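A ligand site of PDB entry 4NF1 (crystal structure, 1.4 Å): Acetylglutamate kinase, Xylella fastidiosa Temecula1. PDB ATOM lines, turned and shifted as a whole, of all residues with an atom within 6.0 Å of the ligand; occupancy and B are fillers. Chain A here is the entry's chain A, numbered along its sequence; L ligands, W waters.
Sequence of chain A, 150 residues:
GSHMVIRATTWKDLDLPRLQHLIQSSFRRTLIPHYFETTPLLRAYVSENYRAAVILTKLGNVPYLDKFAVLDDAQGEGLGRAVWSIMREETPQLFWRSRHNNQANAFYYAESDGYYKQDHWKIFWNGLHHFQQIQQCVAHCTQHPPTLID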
ATOM      1  N   PHE A  27     -31.205  -6.049  -6.331  1.00  0.00           N
ATOM      2  CA  PHE A  27     -30.405  -5.693  -5.164  1.00  0.00           C
ATOM      3  C   PHE A  27     -30.628  -4.248  -4.696  1.00  0.00           C
ATOM      4  O   PHE A  27     -30.192  -3.886  -3.600  1.00  0.00           O
ATOM      5  CB  PHE A  27     -28.913  -5.909  -5.460  1.00  0.00           C
ATOM      6  CG  PHE A  27     -28.493  -7.353  -5.444  1.00  0.00           C
ATOM      7  CD1 PHE A  27     -28.072  -7.960  -4.264  1.00  0.00           C
ATOM      8  CD2 PHE A  27     -28.541  -8.121  -6.590  1.00  0.00           C
ATOM      9  CE1 PHE A  27     -27.686  -9.285  -4.249  1.00  0.00           C
ATOM     10  CE2 PHE A  27     -28.163  -9.469  -6.577  1.00  0.00           C
ATOM     11  CZ  PHE A  27     -27.747 -10.040  -5.397  1.00  0.00           C
ATOM     12  N   ARG A  29     -29.174  -1.680  -5.756  1.00  0.00           N
ATOM     13  CA  ARG A  29     -27.883  -1.016  -5.728  1.00  0.00           C
ATOM     14  C   ARG A  29     -27.286  -0.973  -7.111  1.00  0.00           C
ATOM     15  O   ARG A  29     -27.897  -1.443  -8.074  1.00  0.00           O
ATOM     16  CB  ARG A  29     -26.954  -1.734  -4.744  1.00  0.00           C
ATOM     17  CG  ARG A  29     -27.464  -1.688  -3.308  1.00  0.00           C
ATOM     18  CD  ARG A  29     -26.458  -2.243  -2.365  1.00  0.00           C
ATOM     19  NE  ARG A  29     -25.326  -1.341  -2.236  1.00  0.00           N
ATOM     20  CZ  ARG A  29     -24.136  -1.717  -1.804  1.00  0.00           C
ATOM     21  NH1 ARG A  29     -23.923  -2.988  -1.466  1.00  0.00           N
ATOM     22  NH2 ARG A  29     -23.149  -0.821  -1.712  1.00  0.00           N
ATOM     23  N   TYR A  64     -18.751 -20.938  -7.773  1.00  0.00           N
ATOM     24  CA  TYR A  64     -19.152 -19.867  -6.862  1.00  0.00           C
ATOM     25  C   TYR A  64     -20.402 -19.179  -7.405  1.00  0.00           C
ATOM     26  O   TYR A  64     -20.417 -18.711  -8.549  1.00  0.00           O
ATOM     27  CB  TYR A  64     -18.008 -18.851  -6.686  1.00  0.00           C
ATOM     28  CG  TYR A  64     -18.368 -17.661  -5.826  1.00  0.00           C
ATOM     29  CD1 TYR A  64     -18.724 -17.817  -4.491  1.00  0.00           C
ATOM     30  CD2 TYR A  64     -18.343 -16.350  -6.353  1.00  0.00           C
ATOM     31  CE1 TYR A  64     -19.049 -16.731  -3.707  1.00  0.00           C
ATOM     32  CE2 TYR A  64     -18.669 -15.256  -5.563  1.00  0.00           C
ATOM     33  CZ  TYR A  64     -19.011 -15.446  -4.230  1.00  0.00           C
ATOM     34  OH  TYR A  64     -19.336 -14.369  -3.451  1.00  0.00           O
ATOM     35  N   LEU A  65     -21.472 -19.147  -6.621  1.00  0.00           N
ATOM     36  CA  LEU A  65     -22.680 -18.472  -7.071  1.00  0.00           C
ATOM     37  C   LEU A  65     -22.572 -17.006  -6.703  1.00  0.00           C
ATOM     38  O   LEU A  65     -22.773 -16.610  -5.558  1.00  0.00           O
ATOM     39  CB  LEU A  65     -23.897 -19.125  -6.440  1.00  0.00           C
ATOM     40  CG  LEU A  65     -25.215 -18.901  -7.176  1.00  0.00           C
ATOM     41  CD1 LEU A  65     -26.192 -19.967  -6.740  1.00  0.00           C
ATOM     42  CD2 LEU A  65     -25.784 -17.554  -6.912  1.00  0.00           C
ATOM     43  N   ASP A  66     -22.173 -16.206  -7.685  1.00  0.00           N
ATOM     44  CA  ASP A  66     -21.862 -14.799  -7.467  1.00  0.00           C
ATOM     45  C   ASP A  66     -23.074 -13.896  -7.356  1.00  0.00           C
ATOM     46  O   ASP A  66     -23.043 -12.890  -6.644  1.00  0.00           O
ATOM     47  CB  ASP A  66     -20.964 -14.330  -8.604  1.00  0.00           C
ATOM     48  CG  ASP A  66     -20.519 -12.899  -8.433  1.00  0.00           C
ATOM     49  OD1 ASP A  66     -19.675 -12.663  -7.535  1.00  0.00           O
ATOM     50  OD2 ASP A  66     -21.016 -12.011  -9.173  1.00  0.00           O
ATOM     51  N   LYS A  67     -24.128 -14.243  -8.081  1.00  0.00           N
ATOM     52  CA  LYS A  67     -25.379 -13.478  -8.017  1.00  0.00           C
ATOM     53  C   LYS A  67     -26.602 -14.358  -8.114  1.00  0.00           C
ATOM     54  O   LYS A  67     -26.695 -15.193  -9.016  1.00  0.00           O
ATOM     55  CB  LYS A  67     -25.461 -12.467  -9.168  1.00  0.00           C
ATOM     56  CG  LYS A  67     -24.361 -11.415  -9.250  1.00  0.00           C
ATOM     57  CD  LYS A  67     -24.550 -10.305  -8.221  1.00  0.00           C
ATOM     58  CE  LYS A  67     -23.368  -9.338  -8.205  1.00  0.00           C
ATOM     59  NZ  LYS A  67     -22.158 -10.005  -7.640  1.00  0.00           N
ATOM     60  N   PHE A  68     -27.526 -14.200  -7.166  1.00  0.00           N
ATOM     61  CA  PHE A  68     -28.887 -14.727  -7.296  1.00  0.00           C
ATOM     62  C   PHE A  68     -29.795 -13.513  -7.307  1.00  0.00           C
ATOM     63  O   PHE A  68     -30.060 -12.934  -6.260  1.00  0.00           O
ATOM     64  CB  PHE A  68     -29.228 -15.666  -6.137  1.00  0.00           C
ATOM     65  CG  PHE A  68     -30.592 -16.323  -6.254  1.00  0.00           C
ATOM     66  CD1 PHE A  68     -31.097 -16.735  -7.479  1.00  0.00           C
ATOM     67  CD2 PHE A  68     -31.321 -16.585  -5.111  1.00  0.00           C
ATOM     68  CE1 PHE A  68     -32.337 -17.382  -7.565  1.00  0.00           C
ATOM     69  CE2 PHE A  68     -32.569 -17.230  -5.182  1.00  0.00           C
ATOM     70  CZ  PHE A  68     -33.067 -17.628  -6.411  1.00  0.00           C
ATOM     71  N   ALA A  69     -30.223 -13.105  -8.495  1.00  0.00           N
ATOM     72  CA  ALA A  69     -30.971 -11.863  -8.663  1.00  0.00           C
ATOM     73  C   ALA A  69     -32.389 -12.222  -9.035  1.00  0.00           C
ATOM     74  O   ALA A  69     -32.601 -12.813 -10.095  1.00  0.00           O
ATOM     75  CB  ALA A  69     -30.347 -11.007  -9.750  1.00  0.00           C
ATOM     76  N   TRP A  96     -21.755 -19.965  -1.800  1.00  0.00           N
ATOM     77  CA  TRP A  96     -22.199 -18.586  -2.010  1.00  0.00           C
ATOM     78  C   TRP A  96     -22.315 -17.885  -0.683  1.00  0.00           C
ATOM     79  O   TRP A  96     -22.259 -18.528   0.363  1.00  0.00           O
ATOM     80  CB  TRP A  96     -23.538 -18.543  -2.764  1.00  0.00           C
ATOM     81  CG  TRP A  96     -24.796 -19.006  -2.025  1.00  0.00           C
ATOM     82  CD1 TRP A  96     -25.712 -18.209  -1.387  1.00  0.00           C
ATOM     83  CD2 TRP A  96     -25.289 -20.351  -1.913  1.00  0.00           C
ATOM     84  NE1 TRP A  96     -26.745 -18.991  -0.876  1.00  0.00           N
ATOM     85  CE2 TRP A  96     -26.500 -20.308  -1.191  1.00  0.00           C
ATOM     86  CE3 TRP A  96     -24.813 -21.592  -2.344  1.00  0.00           C
ATOM     87  CZ2 TRP A  96     -27.250 -21.457  -0.902  1.00  0.00           C
ATOM     88  CZ3 TRP A  96     -25.571 -22.737  -2.026  1.00  0.00           C
ATOM     89  CH2 TRP A  96     -26.770 -22.648  -1.337  1.00  0.00           C
ATOM     90  N   ARG A  97     -22.440 -16.568  -0.742  1.00  0.00           N
ATOM     91  CA  ARG A  97     -22.623 -15.764   0.461  1.00  0.00           C
ATOM     92  C   ARG A  97     -23.914 -14.948   0.409  1.00  0.00           C
ATOM     93  O   ARG A  97     -24.479 -14.736  -0.675  1.00  0.00           O
ATOM     94  CB  ARG A  97     -21.412 -14.838   0.686  1.00  0.00           C
ATOM     95  CG  ARG A  97     -21.301 -13.718  -0.346  1.00  0.00           C
ATOM     96  CD  ARG A  97     -19.913 -13.089  -0.312  1.00  0.00           C
ATOM     97  NE  ARG A  97     -19.800 -11.971  -1.249  1.00  0.00           N
ATOM     98  CZ  ARG A  97     -18.687 -11.266  -1.403  1.00  0.00           C
ATOM     99  NH1 ARG A  97     -17.615 -11.545  -0.655  1.00  0.00           N
ATOM    100  NH2 ARG A  97     -18.634 -10.267  -2.273  1.00  0.00           N
ATOM    101  N   SER A  98     -24.380 -14.519   1.578  1.00  0.00           N
ATOM    102  CA  SER A  98     -25.649 -13.812   1.692  1.00  0.00           C
ATOM    103  C   SER A  98     -25.616 -12.871   2.882  1.00  0.00           C
ATOM    104  O   SER A  98     -25.092 -13.196   3.935  1.00  0.00           O
ATOM    105  CB  SER A  98     -26.787 -14.810   1.853  1.00  0.00           C
ATOM    106  OG  SER A  98     -28.041 -14.141   1.880  1.00  0.00           O
ATOM    107  N   ARG A  99     -26.178 -11.670   2.699  1.00  0.00           N
ATOM    108  CA  ARG A  99     -26.364 -10.752   3.819  1.00  0.00           C
ATOM    109  C   ARG A  99     -27.275 -11.358   4.870  1.00  0.00           C
ATOM    110  O   ARG A  99     -28.193 -12.114   4.553  1.00  0.00           O
ATOM    111  CB  ARG A  99     -26.964  -9.436   3.331  1.00  0.00           C
ATOM    112  CG  ARG A  99     -25.992  -8.544   2.576  1.00  0.00           C
ATOM    113  CD  ARG A  99     -26.717  -7.298   2.078  1.00  0.00           C
ATOM    114  NE  ARG A  99     -27.226  -6.486   3.191  1.00  0.00           N
ATOM    115  CZ  ARG A  99     -26.519  -5.549   3.800  1.00  0.00           C
ATOM    116  NH1 ARG A  99     -25.276  -5.295   3.411  1.00  0.00           N
ATOM    117  NH2 ARG A  99     -27.066  -4.859   4.805  1.00  0.00           N
ATOM    118  N   ASN A 102     -31.033 -10.881   4.165  1.00  0.00           N
ATOM    119  CA  ASN A 102     -31.534 -11.254   2.845  1.00  0.00           C
ATOM    120  C   ASN A 102     -32.848 -12.027   2.944  1.00  0.00           C
ATOM    121  O   ASN A 102     -32.909 -13.058   3.626  1.00  0.00           O
ATOM    122  CB  ASN A 102     -30.509 -12.118   2.118  1.00  0.00           C
ATOM    123  CG  ASN A 102     -30.817 -12.313   0.634  1.00  0.00           C
ATOM    124  OD1 ASN A 102     -31.898 -11.960   0.154  1.00  0.00           O
ATOM    125  ND2 ASN A 102     -29.876 -12.881  -0.076  1.00  0.00           N
ATOM    126  N   TYR A 108     -32.401 -20.286   1.127  1.00  0.00           N
ATOM    127  CA  TYR A 108     -31.048 -20.812   1.235  1.00  0.00           C
ATOM    128  C   TYR A 108     -30.915 -21.887   2.322  1.00  0.00           C
ATOM    129  O   TYR A 108     -30.228 -22.890   2.126  1.00  0.00           O
ATOM    130  CB  TYR A 108     -30.077 -19.684   1.519  1.00  0.00           C
ATOM    131  CG  TYR A 108     -29.850 -18.680   0.400  1.00  0.00           C
ATOM    132  CD1 TYR A 108     -30.105 -19.006  -0.938  1.00  0.00           C
ATOM    133  CD2 TYR A 108     -29.339 -17.434   0.692  1.00  0.00           C
ATOM    134  CE1 TYR A 108     -29.868 -18.066  -1.942  1.00  0.00           C
ATOM    135  CE2 TYR A 108     -29.087 -16.509  -0.289  1.00  0.00           C
ATOM    136  CZ  TYR A 108     -29.339 -16.837  -1.605  1.00  0.00           C
ATOM    137  OH  TYR A 108     -29.049 -15.874  -2.568  1.00  0.00           O
ATOM    138  N   HIS A 120     -19.827 -10.669   8.418  1.00  0.00           N
ATOM    139  CA  HIS A 120     -20.581  -9.935   7.385  1.00  0.00           C
ATOM    140  C   HIS A 120     -21.658 -10.848   6.840  1.00  0.00           C
ATOM    141  O   HIS A 120     -22.772 -10.429   6.494  1.00  0.00           O
ATOM    142  CB  HIS A 120     -19.802  -9.611   6.115  1.00  0.00           C
ATOM    143  CG  HIS A 120     -20.535  -8.671   5.226  1.00  0.00           C
ATOM    144  ND1 HIS A 120     -20.666  -8.856   3.883  1.00  0.00           N
ATOM    145  CD2 HIS A 120     -20.751  -7.356   5.437  1.00  0.00           C
ATOM    146  CE1 HIS A 120     -21.269  -7.794   3.363  1.00  0.00           C
ATOM    147  NE2 HIS A 120     -21.297  -6.865   4.278  1.00  0.00           N
ATOM    148  N   TRP A 121     -21.232 -12.078   6.607  1.00  0.00           N
ATOM    149  CA  TRP A 121     -21.933 -12.930   5.689  1.00  0.00           C
ATOM    150  C   TRP A 121     -22.438 -14.196   6.315  1.00  0.00           C
ATOM    151  O   TRP A 121     -21.821 -14.748   7.226  1.00  0.00           O
ATOM    152  CB  TRP A 121     -21.025 -13.325   4.517  1.00  0.00           C
ATOM    153  CG  TRP A 121     -20.432 -12.253   3.663  1.00  0.00           C
ATOM    154  CD1 TRP A 121     -19.111 -11.934   3.580  1.00  0.00           C
ATOM    155  CD2 TRP A 121     -21.106 -11.434   2.707  1.00  0.00           C
ATOM    156  NE1 TRP A 121     -18.934 -10.920   2.659  1.00  0.00           N
ATOM    157  CE2 TRP A 121     -20.140 -10.627   2.080  1.00  0.00           C
ATOM    158  CE3 TRP A 121     -22.453 -11.303   2.327  1.00  0.00           C
ATOM    159  CZ2 TRP A 121     -20.469  -9.665   1.114  1.00  0.00           C
ATOM    160  CZ3 TRP A 121     -22.777 -10.369   1.366  1.00  0.00           C
ATOM    161  CH2 TRP A 121     -21.798  -9.552   0.779  1.00  0.00           C
ATOM    162  N   HIS A 144     -13.426 -12.086  -0.766  1.00  0.00           N
ATOM    163  CA  HIS A 144     -13.764 -11.654  -2.112  1.00  0.00           C
ATOM    164  C   HIS A 144     -14.362 -10.243  -2.127  1.00  0.00           C
ATOM    165  O   HIS A 144     -15.328  -9.980  -1.430  1.00  0.00           O
ATOM    166  CB  HIS A 144     -14.738 -12.646  -2.729  1.00  0.00           C
ATOM    167  CG  HIS A 144     -14.935 -12.495  -4.202  1.00  0.00           C
ATOM    168  ND1 HIS A 144     -13.889 -12.614  -5.112  1.00  0.00           N
ATOM    169  CD2 HIS A 144     -16.040 -12.270  -4.943  1.00  0.00           C
ATOM    170  CE1 HIS A 144     -14.362 -12.460  -6.336  1.00  0.00           C
ATOM    171  NE2 HIS A 144     -15.668 -12.241  -6.267  1.00  0.00           N
ATOM    172  N   THR A 147     -19.030  -6.418  -5.393  1.00  0.00           N
ATOM    173  CA  THR A 147     -19.312  -5.968  -6.762  1.00  0.00           C
ATOM    174  C   THR A 147     -20.616  -5.162  -6.855  1.00  0.00           C
ATOM    175  O   THR A 147     -21.083  -4.860  -7.959  1.00  0.00           O
ATOM    176  CB  THR A 147     -19.341  -7.158  -7.740  1.00  0.00           C
ATOM    177  OG1 THR A 147     -20.054  -8.251  -7.155  1.00  0.00           O
ATOM    178  CG2 THR A 147     -17.914  -7.589  -8.044  1.00  0.00           C
ATOM    179  N   LEU A 148     -21.204  -4.834  -5.704  1.00  0.00           N
ATOM    180  CA  LEU A 148     -22.298  -3.866  -5.646  1.00  0.00           C
ATOM    181  C   LEU A 148     -21.817  -2.624  -4.915  1.00  0.00           C
ATOM    182  O   LEU A 148     -21.065  -2.729  -3.943  1.00  0.00           O
ATOM    183  CB  LEU A 148     -23.514  -4.452  -4.935  1.00  0.00           C
ATOM    184  CG  LEU A 148     -24.100  -5.657  -5.657  1.00  0.00           C
ATOM    185  CD1 LEU A 148     -25.108  -6.394  -4.794  1.00  0.00           C
ATOM    186  CD2 LEU A 148     -24.719  -5.225  -6.986  1.00  0.00           C
HETATM  187  C1  LIG L   1     -24.147 -11.494  -3.824  1.00  0.00           C
HETATM  188  C2  LIG L   1     -22.700 -11.177  -4.042  1.00  0.00           C
HETATM  189  O1  LIG L   1     -21.783 -11.812  -3.436  1.00  0.00           O
HETATM  190  O2  LIG L   1     -22.345 -10.270  -4.861  1.00  0.00           O
HETATM  191  C3  LIG L   1     -24.591 -10.817  -2.557  1.00  0.00           C
HETATM  192  C4  LIG L   1     -24.259  -9.344  -2.530  1.00  0.00           C
HETATM  193  C5  LIG L   1     -24.842  -8.466  -1.468  1.00  0.00           C
HETATM  194  O3  LIG L   1     -25.848  -8.864  -0.844  1.00  0.00           O
HETATM  195  O4  LIG L   1     -24.328  -7.348  -1.200  1.00  0.00           O
HETATM  196  C6  LIG L   1     -25.477 -13.597  -4.203  1.00  0.00           C
HETATM  197  C7  LIG L   1     -25.557 -15.101  -4.021  1.00  0.00           C
HETATM  198  O5  LIG L   1     -26.376 -12.951  -4.732  1.00  0.00           O
HETATM  199  N1  LIG L   1     -24.303 -12.924  -3.688  1.00  0.00           N
HETATM  200  O   HOH W   1     -19.613 -12.035  -4.909  1.00  0.00           O
HETATM  201  O   HOH W   2     -22.023  -6.598  -2.318  1.00  0.00           O
HETATM  202  O   HOH W   3     -25.793  -5.125  -1.194  1.00  0.00           O
HETATM  203  O   HOH W   4     -27.120 -13.926  -1.462  1.00  0.00           O
HETATM  204  O   HOH W   5     -27.161 -11.113  -0.076  1.00  0.00           O
HETATM  205  O   HOH W   6     -29.045 -12.769  -3.504  1.00  0.00           O
HETATM  206  O   HOH W   7     -20.605  -8.462  -3.774  1.00  0.00           O
HETATM  207  O   HOH W   8     -28.048  -7.228  -0.620  1.00  0.00           O
HETATM  208  O   HOH W   9     -22.200 -15.162  -3.355  1.00  0.00           O
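OD2 of Asp 66 lies within salt-bridge range of NZ of Lys 67. The side-chain hydroxyl (OG1) of Thr 147 lies within hydrogen-bond range of the side-chain amino group (NZ) of Lys 67 (2.8 Å). The guanidinium group of Arg 97 lies within hydrogen-bond range of the side-chain hydroxyl of Tyr 64 (3.3 Å). The guanidinium group (NH1) of Arg 97 is in hydrogen-bond range of the backbone carbonyl oxygen (O) of His 144 (2.9 Å). The indole nitrogen (NE1) of Trp 121 lies close to a ring nitrogen (ND1) of His 120.
Residues that only touch the ligand: Phe 27 (3.3 Å), Arg 99 (3.4 Å), Leu 65 (3.5 Å), Tyr 64 (3.5 Å), Leu 148 (3.8 Å), Thr 147 (3.8 Å), Tyr 108 (3.9 Å) and Trp 121 (3.9 Å). Of the 19 residues printed, 12 come within 4 Å of the ligand. Along chain A the residues within 4 Å of the ligand span positions 27 to 148. The nearest printed residue that does not touch the ligand is Trp 96 (4.1 Å).
An oxygen (O2) of the ligand lies within salt-bridge range of the side-chain amino group of Lys 67, 2.8 Å away. O1 of the ligand is in salt-bridge range of NE of Arg 97, 3.0 Å away. O5 of the ligand sits at hydrogen-bond distance from N of Phe 68 (3.0 Å). N1 of the ligand lies close to O of Asp 66 (3.2 Å).
Water W1 lies within hydrogen-bond range of an oxygen (O1) of the ligand, the side-chain carboxylate of Asp 66, the side-chain hydroxyl of Tyr 64 and the guanidinium group of Arg 97. Water W3 bridges O4 of the ligand (2.7 Å) and NH1 of Arg 29 (2.9 Å). Water W5 lies within hydrogen-bond range of an oxygen (O3) of the ligand (2.7 Å), the backbone NH (N) of Arg 99 (3.0 Å) and the side-chain amide nitrogen (ND2) of Asn 102 (3.2 Å). Water W7 lies within hydrogen-bond range of an oxygen (O2) of the ligand (2.7 Å), the backbone NH of Thr 147 (3.0 Å) and the guanidinium group of Arg 97 (3.1 Å). Water W6 lies within hydrogen-bond range of O of Phe 68 (2.9 Å), O5 of the ligand (2.9 Å) and OH of Tyr 108 (3.2 Å). Water W9 lies within hydrogen-bond range of the backbone carbonyl oxygen of Leu 65, the side-chain hydroxyl of Tyr 64, the backbone NH of Arg 97 and a nitrogen (N1) of the ligand.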
